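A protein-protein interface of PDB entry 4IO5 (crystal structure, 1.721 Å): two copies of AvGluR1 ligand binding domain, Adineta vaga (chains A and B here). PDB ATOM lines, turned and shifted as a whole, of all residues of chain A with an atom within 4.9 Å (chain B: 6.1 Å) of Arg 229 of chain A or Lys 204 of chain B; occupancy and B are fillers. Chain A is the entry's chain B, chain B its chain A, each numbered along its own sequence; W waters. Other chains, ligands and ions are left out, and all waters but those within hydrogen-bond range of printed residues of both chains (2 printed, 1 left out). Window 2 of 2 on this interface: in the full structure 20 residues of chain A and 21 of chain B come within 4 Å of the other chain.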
ATOM      1  N   ASN A 100       9.807  19.171 -16.507  1.00  0.00           N
ATOM      2  CA  ASN A 100      10.236  20.550 -16.334  1.00  0.00           C
ATOM      3  C   ASN A 100      11.223  20.633 -15.196  1.00  0.00           C
ATOM      4  O   ASN A 100      11.151  19.875 -14.230  1.00  0.00           O
ATOM      5  CB  ASN A 100       9.045  21.460 -16.059  1.00  0.00           C
ATOM      6  CG  ASN A 100       8.237  21.690 -17.308  1.00  0.00           C
ATOM      7  OD1 ASN A 100       7.197  21.068 -17.517  1.00  0.00           O
ATOM      8  ND2 ASN A 100       8.748  22.545 -18.184  1.00  0.00           N
ATOM      9  N   SER A 101      12.169  21.542 -15.318  1.00  0.00           N
ATOM     10  CA  SER A 101      13.231  21.629 -14.338  1.00  0.00           C
ATOM     11  C   SER A 101      12.710  21.972 -12.955  1.00  0.00           C
ATOM     12  O   SER A 101      11.815  22.804 -12.789  1.00  0.00           O
ATOM     13  CB  SER A 101      14.292  22.624 -14.777  1.00  0.00           C
ATOM     14  OG  SER A 101      13.728  23.871 -15.069  1.00  0.00           O
ATOM     15  N   ILE A 225       4.729  20.183 -11.252  1.00  0.00           N
ATOM     16  CA  ILE A 225       6.024  20.775 -10.914  1.00  0.00           C
ATOM     17  C   ILE A 225       5.991  22.284 -11.134  1.00  0.00           C
ATOM     18  O   ILE A 225       6.488  23.069 -10.335  1.00  0.00           O
ATOM     19  CB  ILE A 225       7.123  20.189 -11.792  1.00  0.00           C
ATOM     20  CG1 ILE A 225       7.411  18.776 -11.346  1.00  0.00           C
ATOM     21  CG2 ILE A 225       8.395  20.967 -11.684  1.00  0.00           C
ATOM     22  CD1 ILE A 225       8.208  18.029 -12.381  1.00  0.00           C
ATOM     23  N   LEU A 226       5.392  22.686 -12.246  1.00  0.00           N
ATOM     24  CA  LEU A 226       5.350  24.095 -12.576  1.00  0.00           C
ATOM     25  C   LEU A 226       4.518  24.830 -11.544  1.00  0.00           C
ATOM     26  O   LEU A 226       4.825  25.966 -11.184  1.00  0.00           O
ATOM     27  CB  LEU A 226       4.811  24.294 -13.996  1.00  0.00           C
ATOM     28  CG  LEU A 226       5.793  23.914 -15.108  1.00  0.00           C
ATOM     29  CD1 LEU A 226       5.096  23.734 -16.455  1.00  0.00           C
ATOM     30  CD2 LEU A 226       6.926  24.960 -15.229  1.00  0.00           C
ATOM     31  N   SER A 227       3.466  24.177 -11.051  1.00  0.00           N
ATOM     32  CA  SER A 227       2.623  24.785 -10.033  1.00  0.00           C
ATOM     33  C   SER A 227       3.397  24.959  -8.733  1.00  0.00           C
ATOM     34  O   SER A 227       3.286  25.993  -8.069  1.00  0.00           O
ATOM     35  CB  SER A 227       1.325  24.001  -9.818  1.00  0.00           C
ATOM     36  OG  SER A 227       0.557  24.591  -8.770  1.00  0.00           O
ATOM     37  N   LEU A 228       4.195  23.961  -8.365  1.00  0.00           N
ATOM     38  CA  LEU A 228       5.042  24.098  -7.171  1.00  0.00           C
ATOM     39  C   LEU A 228       6.049  25.229  -7.343  1.00  0.00           C
ATOM     40  O   LEU A 228       6.349  25.928  -6.387  1.00  0.00           O
ATOM     41  CB  LEU A 228       5.759  22.797  -6.800  1.00  0.00           C
ATOM     42  CG  LEU A 228       4.853  21.614  -6.459  1.00  0.00           C
ATOM     43  CD1 LEU A 228       5.693  20.385  -6.335  1.00  0.00           C
ATOM     44  CD2 LEU A 228       4.112  21.867  -5.159  1.00  0.00           C
ATOM     45  N   ARG A 229       6.585  25.405  -8.554  1.00  0.00           N
ATOM     46  CA  ARG A 229       7.504  26.482  -8.829  1.00  0.00           C
ATOM     47  C   ARG A 229       6.784  27.817  -8.634  1.00  0.00           C
ATOM     48  O   ARG A 229       7.265  28.697  -7.907  1.00  0.00           O
ATOM     49  CB  ARG A 229       8.043  26.344 -10.266  1.00  0.00           C
ATOM     50  CG  ARG A 229       8.836  27.527 -10.831  1.00  0.00           C
ATOM     51  CD  ARG A 229       9.030  27.425 -12.396  1.00  0.00           C
ATOM     52  NE  ARG A 229       9.764  26.219 -12.834  1.00  0.00           N
ATOM     53  CZ  ARG A 229      10.223  25.997 -14.078  1.00  0.00           C
ATOM     54  NH1 ARG A 229      10.048  26.880 -15.056  1.00  0.00           N
ATOM     55  NH2 ARG A 229      10.877  24.873 -14.354  1.00  0.00           N
ATOM     56  N   GLU A 230       5.629  27.951  -9.281  1.00  0.00           N
ATOM     57  CA  GLU A 230       4.920  29.229  -9.344  1.00  0.00           C
ATOM     58  C   GLU A 230       4.447  29.692  -7.988  1.00  0.00           C
ATOM     59  O   GLU A 230       4.463  30.886  -7.691  1.00  0.00           O
ATOM     60  CB  GLU A 230       3.727  29.110 -10.292  1.00  0.00           C
ATOM     61  CG  GLU A 230       4.172  29.038 -11.724  1.00  0.00           C
ATOM     62  CD  GLU A 230       3.143  28.473 -12.678  1.00  0.00           C
ATOM     63  OE1 GLU A 230       1.987  28.282 -12.287  1.00  0.00           O
ATOM     64  OE2 GLU A 230       3.532  28.197 -13.841  1.00  0.00           O
ATOM     65  N   THR A 231       4.032  28.745  -7.165  1.00  0.00           N
ATOM     66  CA  THR A 231       3.517  29.080  -5.850  1.00  0.00           C
ATOM     67  C   THR A 231       4.591  29.150  -4.766  1.00  0.00           C
ATOM     68  O   THR A 231       4.261  29.334  -3.592  1.00  0.00           O
ATOM     69  CB  THR A 231       2.407  28.112  -5.411  1.00  0.00           C
ATOM     70  OG1 THR A 231       2.920  26.789  -5.284  1.00  0.00           O
ATOM     71  CG2 THR A 231       1.247  28.096  -6.393  1.00  0.00           C
ATOM     72  N   GLY A 232       5.865  29.021  -5.143  1.00  0.00           N
ATOM     73  CA  GLY A 232       6.962  29.200  -4.215  1.00  0.00           C
ATOM     74  C   GLY A 232       7.336  28.005  -3.341  1.00  0.00           C
ATOM     75  O   GLY A 232       8.203  28.124  -2.479  1.00  0.00           O
ATOM     76  N   ILE A 233       6.721  26.851  -3.577  1.00  0.00           N
ATOM     77  CA  ILE A 233       6.997  25.664  -2.771  1.00  0.00           C
ATOM     78  C   ILE A 233       8.442  25.168  -2.974  1.00  0.00           C
ATOM     79  O   ILE A 233       9.125  24.814  -2.001  1.00  0.00           O
ATOM     80  CB  ILE A 233       6.005  24.533  -3.080  1.00  0.00           C
ATOM     81  CG1 ILE A 233       4.578  24.912  -2.687  1.00  0.00           C
ATOM     82  CG2 ILE A 233       6.457  23.246  -2.440  1.00  0.00           C
ATOM     83  CD1 ILE A 233       4.444  25.382  -1.308  1.00  0.00           C
ATOM     84  N   LEU A 234       8.918  25.151  -4.221  1.00  0.00           N
ATOM     85  CA  LEU A 234      10.286  24.741  -4.483  1.00  0.00           C
ATOM     86  C   LEU A 234      11.286  25.700  -3.810  1.00  0.00           C
ATOM     87  O   LEU A 234      12.274  25.266  -3.252  1.00  0.00           O
ATOM     88  CB  LEU A 234      10.560  24.599  -6.000  1.00  0.00           C
ATOM     89  CG  LEU A 234       9.752  23.535  -6.756  1.00  0.00           C
ATOM     90  CD1 LEU A 234      10.214  23.398  -8.196  1.00  0.00           C
ATOM     91  CD2 LEU A 234       9.822  22.196  -6.052  1.00  0.00           C
ATOM     92  N   VAL B  88       7.572  29.220 -19.635  1.00  0.00           N
ATOM     93  CA  VAL B  88       6.926  27.942 -19.397  1.00  0.00           C
ATOM     94  C   VAL B  88       6.053  28.109 -18.163  1.00  0.00           C
ATOM     95  O   VAL B  88       6.554  28.405 -17.072  1.00  0.00           O
ATOM     96  CB  VAL B  88       7.975  26.821 -19.193  1.00  0.00           C
ATOM     97  CG1 VAL B  88       7.268  25.468 -18.964  1.00  0.00           C
ATOM     98  CG2 VAL B  88       8.918  26.742 -20.368  1.00  0.00           C
ATOM     99  N   ASN B 105      14.989  32.486 -16.563  1.00  0.00           N
ATOM    100  CA  ASN B 105      14.290  33.763 -16.634  1.00  0.00           C
ATOM    101  C   ASN B 105      13.814  34.156 -15.265  1.00  0.00           C
ATOM    102  O   ASN B 105      13.660  33.307 -14.382  1.00  0.00           O
ATOM    103  CB  ASN B 105      13.072  33.649 -17.580  1.00  0.00           C
ATOM    104  CG  ASN B 105      12.335  34.981 -17.771  1.00  0.00           C
ATOM    105  OD1 ASN B 105      12.952  36.006 -18.107  1.00  0.00           O
ATOM    106  ND2 ASN B 105      11.006  34.971 -17.541  1.00  0.00           N
ATOM    107  N   SER B 106      13.566  35.446 -15.118  1.00  0.00           N
ATOM    108  CA  SER B 106      12.862  35.990 -13.966  1.00  0.00           C
ATOM    109  C   SER B 106      12.353  37.358 -14.381  1.00  0.00           C
ATOM    110  O   SER B 106      12.701  37.842 -15.454  1.00  0.00           O
ATOM    111  CB  SER B 106      13.811  36.139 -12.775  1.00  0.00           C
ATOM    112  OG  SER B 106      14.935  36.931 -13.141  1.00  0.00           O
ATOM    113  N   MET B 107      11.554  37.994 -13.532  1.00  0.00           N
ATOM    114  CA  MET B 107      10.994  39.295 -13.873  1.00  0.00           C
ATOM    115  C   MET B 107      11.506  40.346 -12.943  1.00  0.00           C
ATOM    116  O   MET B 107      11.928  40.050 -11.832  1.00  0.00           O
ATOM    117  CB  MET B 107       9.470  39.283 -13.832  1.00  0.00           C
ATOM    118  CG  MET B 107       8.848  38.380 -14.885  1.00  0.00           C
ATOM    119  SD  MET B 107       7.065  38.632 -15.103  1.00  0.00           S
ATOM    120  CE  MET B 107       6.450  37.383 -13.985  1.00  0.00           C
ATOM    121  N   ASP B 201      14.631  40.241  -8.232  1.00  0.00           N
ATOM    122  CA  ASP B 201      13.919  39.583  -9.318  1.00  0.00           C
ATOM    123  C   ASP B 201      12.934  38.592  -8.718  1.00  0.00           C
ATOM    124  O   ASP B 201      13.090  38.133  -7.580  1.00  0.00           O
ATOM    125  CB  ASP B 201      14.869  38.961 -10.359  1.00  0.00           C
ATOM    126  CG  ASP B 201      15.696  37.826  -9.813  1.00  0.00           C
ATOM    127  OD1 ASP B 201      15.725  37.640  -8.579  1.00  0.00           O
ATOM    128  OD2 ASP B 201      16.328  37.113 -10.629  1.00  0.00           O
ATOM    129  N   PHE B 202      11.880  38.312  -9.463  1.00  0.00           N
ATOM    130  CA  PHE B 202      10.824  37.445  -8.980  1.00  0.00           C
ATOM    131  C   PHE B 202      10.321  36.532 -10.088  1.00  0.00           C
ATOM    132  O   PHE B 202      10.664  36.713 -11.268  1.00  0.00           O
ATOM    133  CB  PHE B 202       9.671  38.266  -8.411  1.00  0.00           C
ATOM    134  CG  PHE B 202       9.103  39.285  -9.364  1.00  0.00           C
ATOM    135  CD1 PHE B 202       9.733  40.508  -9.554  1.00  0.00           C
ATOM    136  CD2 PHE B 202       7.916  39.041 -10.029  1.00  0.00           C
ATOM    137  CE1 PHE B 202       9.204  41.451 -10.426  1.00  0.00           C
ATOM    138  CE2 PHE B 202       7.382  39.978 -10.902  1.00  0.00           C
ATOM    139  CZ  PHE B 202       8.027  41.192 -11.097  1.00  0.00           C
ATOM    140  N   ASP B 203       9.545  35.532  -9.687  1.00  0.00           N
ATOM    141  CA  ASP B 203       8.980  34.553 -10.614  1.00  0.00           C
ATOM    142  C   ASP B 203      10.052  33.895 -11.452  1.00  0.00           C
ATOM    143  O   ASP B 203       9.991  33.872 -12.692  1.00  0.00           O
ATOM    144  CB  ASP B 203       7.900  35.226 -11.483  1.00  0.00           C
ATOM    145  CG  ASP B 203       6.926  34.239 -12.083  1.00  0.00           C
ATOM    146  OD1 ASP B 203       6.562  33.268 -11.395  1.00  0.00           O
ATOM    147  OD2 ASP B 203       6.524  34.432 -13.261  1.00  0.00           O
ATOM    148  N   LYS B 204      11.059  33.350 -10.764  1.00  0.00           N
ATOM    149  CA  LYS B 204      12.070  32.522 -11.419  1.00  0.00           C
ATOM    150  C   LYS B 204      11.352  31.484 -12.274  1.00  0.00           C
ATOM    151  O   LYS B 204      10.432  30.811 -11.822  1.00  0.00           O
ATOM    152  CB  LYS B 204      12.959  31.829 -10.392  1.00  0.00           C
ATOM    153  CG  LYS B 204      13.644  32.755  -9.397  1.00  0.00           C
ATOM    154  CD  LYS B 204      14.539  33.778 -10.072  1.00  0.00           C
ATOM    155  CE  LYS B 204      15.507  34.428  -9.077  1.00  0.00           C
ATOM    156  NZ  LYS B 204      14.979  34.456  -7.676  1.00  0.00           N
ATOM    157  N   SER B 205      11.774  31.386 -13.527  1.00  0.00           N
ATOM    158  CA  SER B 205      11.098  30.581 -14.510  1.00  0.00           C
ATOM    159  C   SER B 205      12.081  30.208 -15.621  1.00  0.00           C
ATOM    160  O   SER B 205      13.301  30.377 -15.479  1.00  0.00           O
ATOM    161  CB  SER B 205       9.913  31.349 -15.079  1.00  0.00           C
ATOM    162  OG  SER B 205      10.297  32.647 -15.495  1.00  0.00           O
ATOM    163  N   THR B 206      11.536  29.675 -16.719  1.00  0.00           N
ATOM    164  CA  THR B 206      12.361  29.294 -17.855  1.00  0.00           C
ATOM    165  C   THR B 206      11.649  29.662 -19.137  1.00  0.00           C
ATOM    166  O   THR B 206      10.439  29.843 -19.123  1.00  0.00           O
ATOM    167  CB  THR B 206      12.615  27.770 -17.901  1.00  0.00           C
ATOM    168  OG1 THR B 206      11.365  27.068 -17.897  1.00  0.00           O
ATOM    169  CG2 THR B 206      13.443  27.310 -16.688  1.00  0.00           C
HETATM  170  O   HOH W   1       6.160  33.297  -8.892  1.00  0.00           O
HETATM  171  O   HOH W   2       6.151  29.570 -14.419  1.00  0.00           O
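The backbone NH of Val 88 of chain B is in hydrogen-bond range of the backbone carbonyl oxygen of Thr 206 of chain B (3.0 Å).
The backbone carbonyl oxygen (O) of Asn 105 of chain B sits at hydrogen-bond distance from the backbone NH (N) of Ser 205 of chain B (2.8 Å).
NZ of Lys 204 of chain B is in salt-bridge range of OD1 of Asp 201 of chain B, at 3.4 Å.
O of Asp 203 of chain B sits at hydrogen-bond distance from OG of Ser 205 of chain B.
The backbone carbonyl oxygen of Ser 101 of chain A sits at hydrogen-bond distance from the guanidinium group of Arg 229 of chain A (2.8 Å).
Among the printed residues, pairs that only touch across the chains: Asn 100 of chain A with Val 88 of chain B (3.4 Å), Ser 101 of chain A with Thr 206 of chain B (3.8 Å), Leu 226 of chain A with Val 88 of chain B (3.7 Å), Arg 229 of chain A with Lys 204 of chain B (3.7 Å) and Arg 229 of chain A with Ser 205 of chain B (3.9 Å).
Of the printed residues of chain B, Asn 100 of chain A touches Val 88 (3.4 Å).
Printed residues of chain B within 4 Å of Ser 101 of chain A: Thr 206 (3.8 Å).
Of the printed residues of chain B, Leu 226 of chain A touches Val 88.
Of chain B, only Lys 204 (3.7 Å), Ser 205 (3.9 Å) and Thr 206 (3.1 Å) come within 4 Å of Arg 229 of chain A.
Asn 105 of chain B touches none of the printed residues of chain A.
Ser 106 of chain B touches none of the printed residues of chain A.
Of chain A, only Arg 229 (3.7 Å) comes within 4 Å of Lys 204 of chain B.
Of the printed residues of chain A, Ser 205 of chain B touches Arg 229 (3.9 Å).
Of the printed residues of chain A, Thr 206 of chain B touches Ser 101 and Arg 229.
The nearest printed residue of chain A that does not touch Lys 204 of chain B is Glu 230 of chain A (6.1 Å).
The nearest printed residue of chain B that does not touch Asn 100 of chain A is Thr 206 of chain B (5.2 Å).
The guanidinium group of Arg 229 of chain A lies within hydrogen-bond range of the side-chain hydroxyl of Thr 206 of chain B (3.1 Å).
Water W1 bridges the side-chain carboxylate (OD1) of Asp 203 of chain B and the backbone carbonyl oxygen (O) of Glu 230 of chain A.
Water W2 lies within hydrogen-bond range of O of Val 88 of chain B (2.9 Å) and OE2 of Glu 230 of chain A (3.0 Å).
Of the 10 printed residues of chain B, 4 touch a printed residue of chain A.
Hydrophobic or aromatic side chains of chain B within 4 Å of the printed part of chain A: Val 88.
Of the 12 printed residues of chain A, 4 touch a printed residue of chain B.
Hydrophobic or aromatic side chains of chain A within 4 Å of the printed part of chain B: Leu 226.
Along chain A the printed residues that touch a printed residue of chain B span positions 100 to 229.
Among the printed residues, 6 pairs touch across the chains.
Among the printed residues, no Asp or Glu carboxylate lies within 4 Å of a Lys or Arg side-chain nitrogen of the other chain.
No position is printed for both chains.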
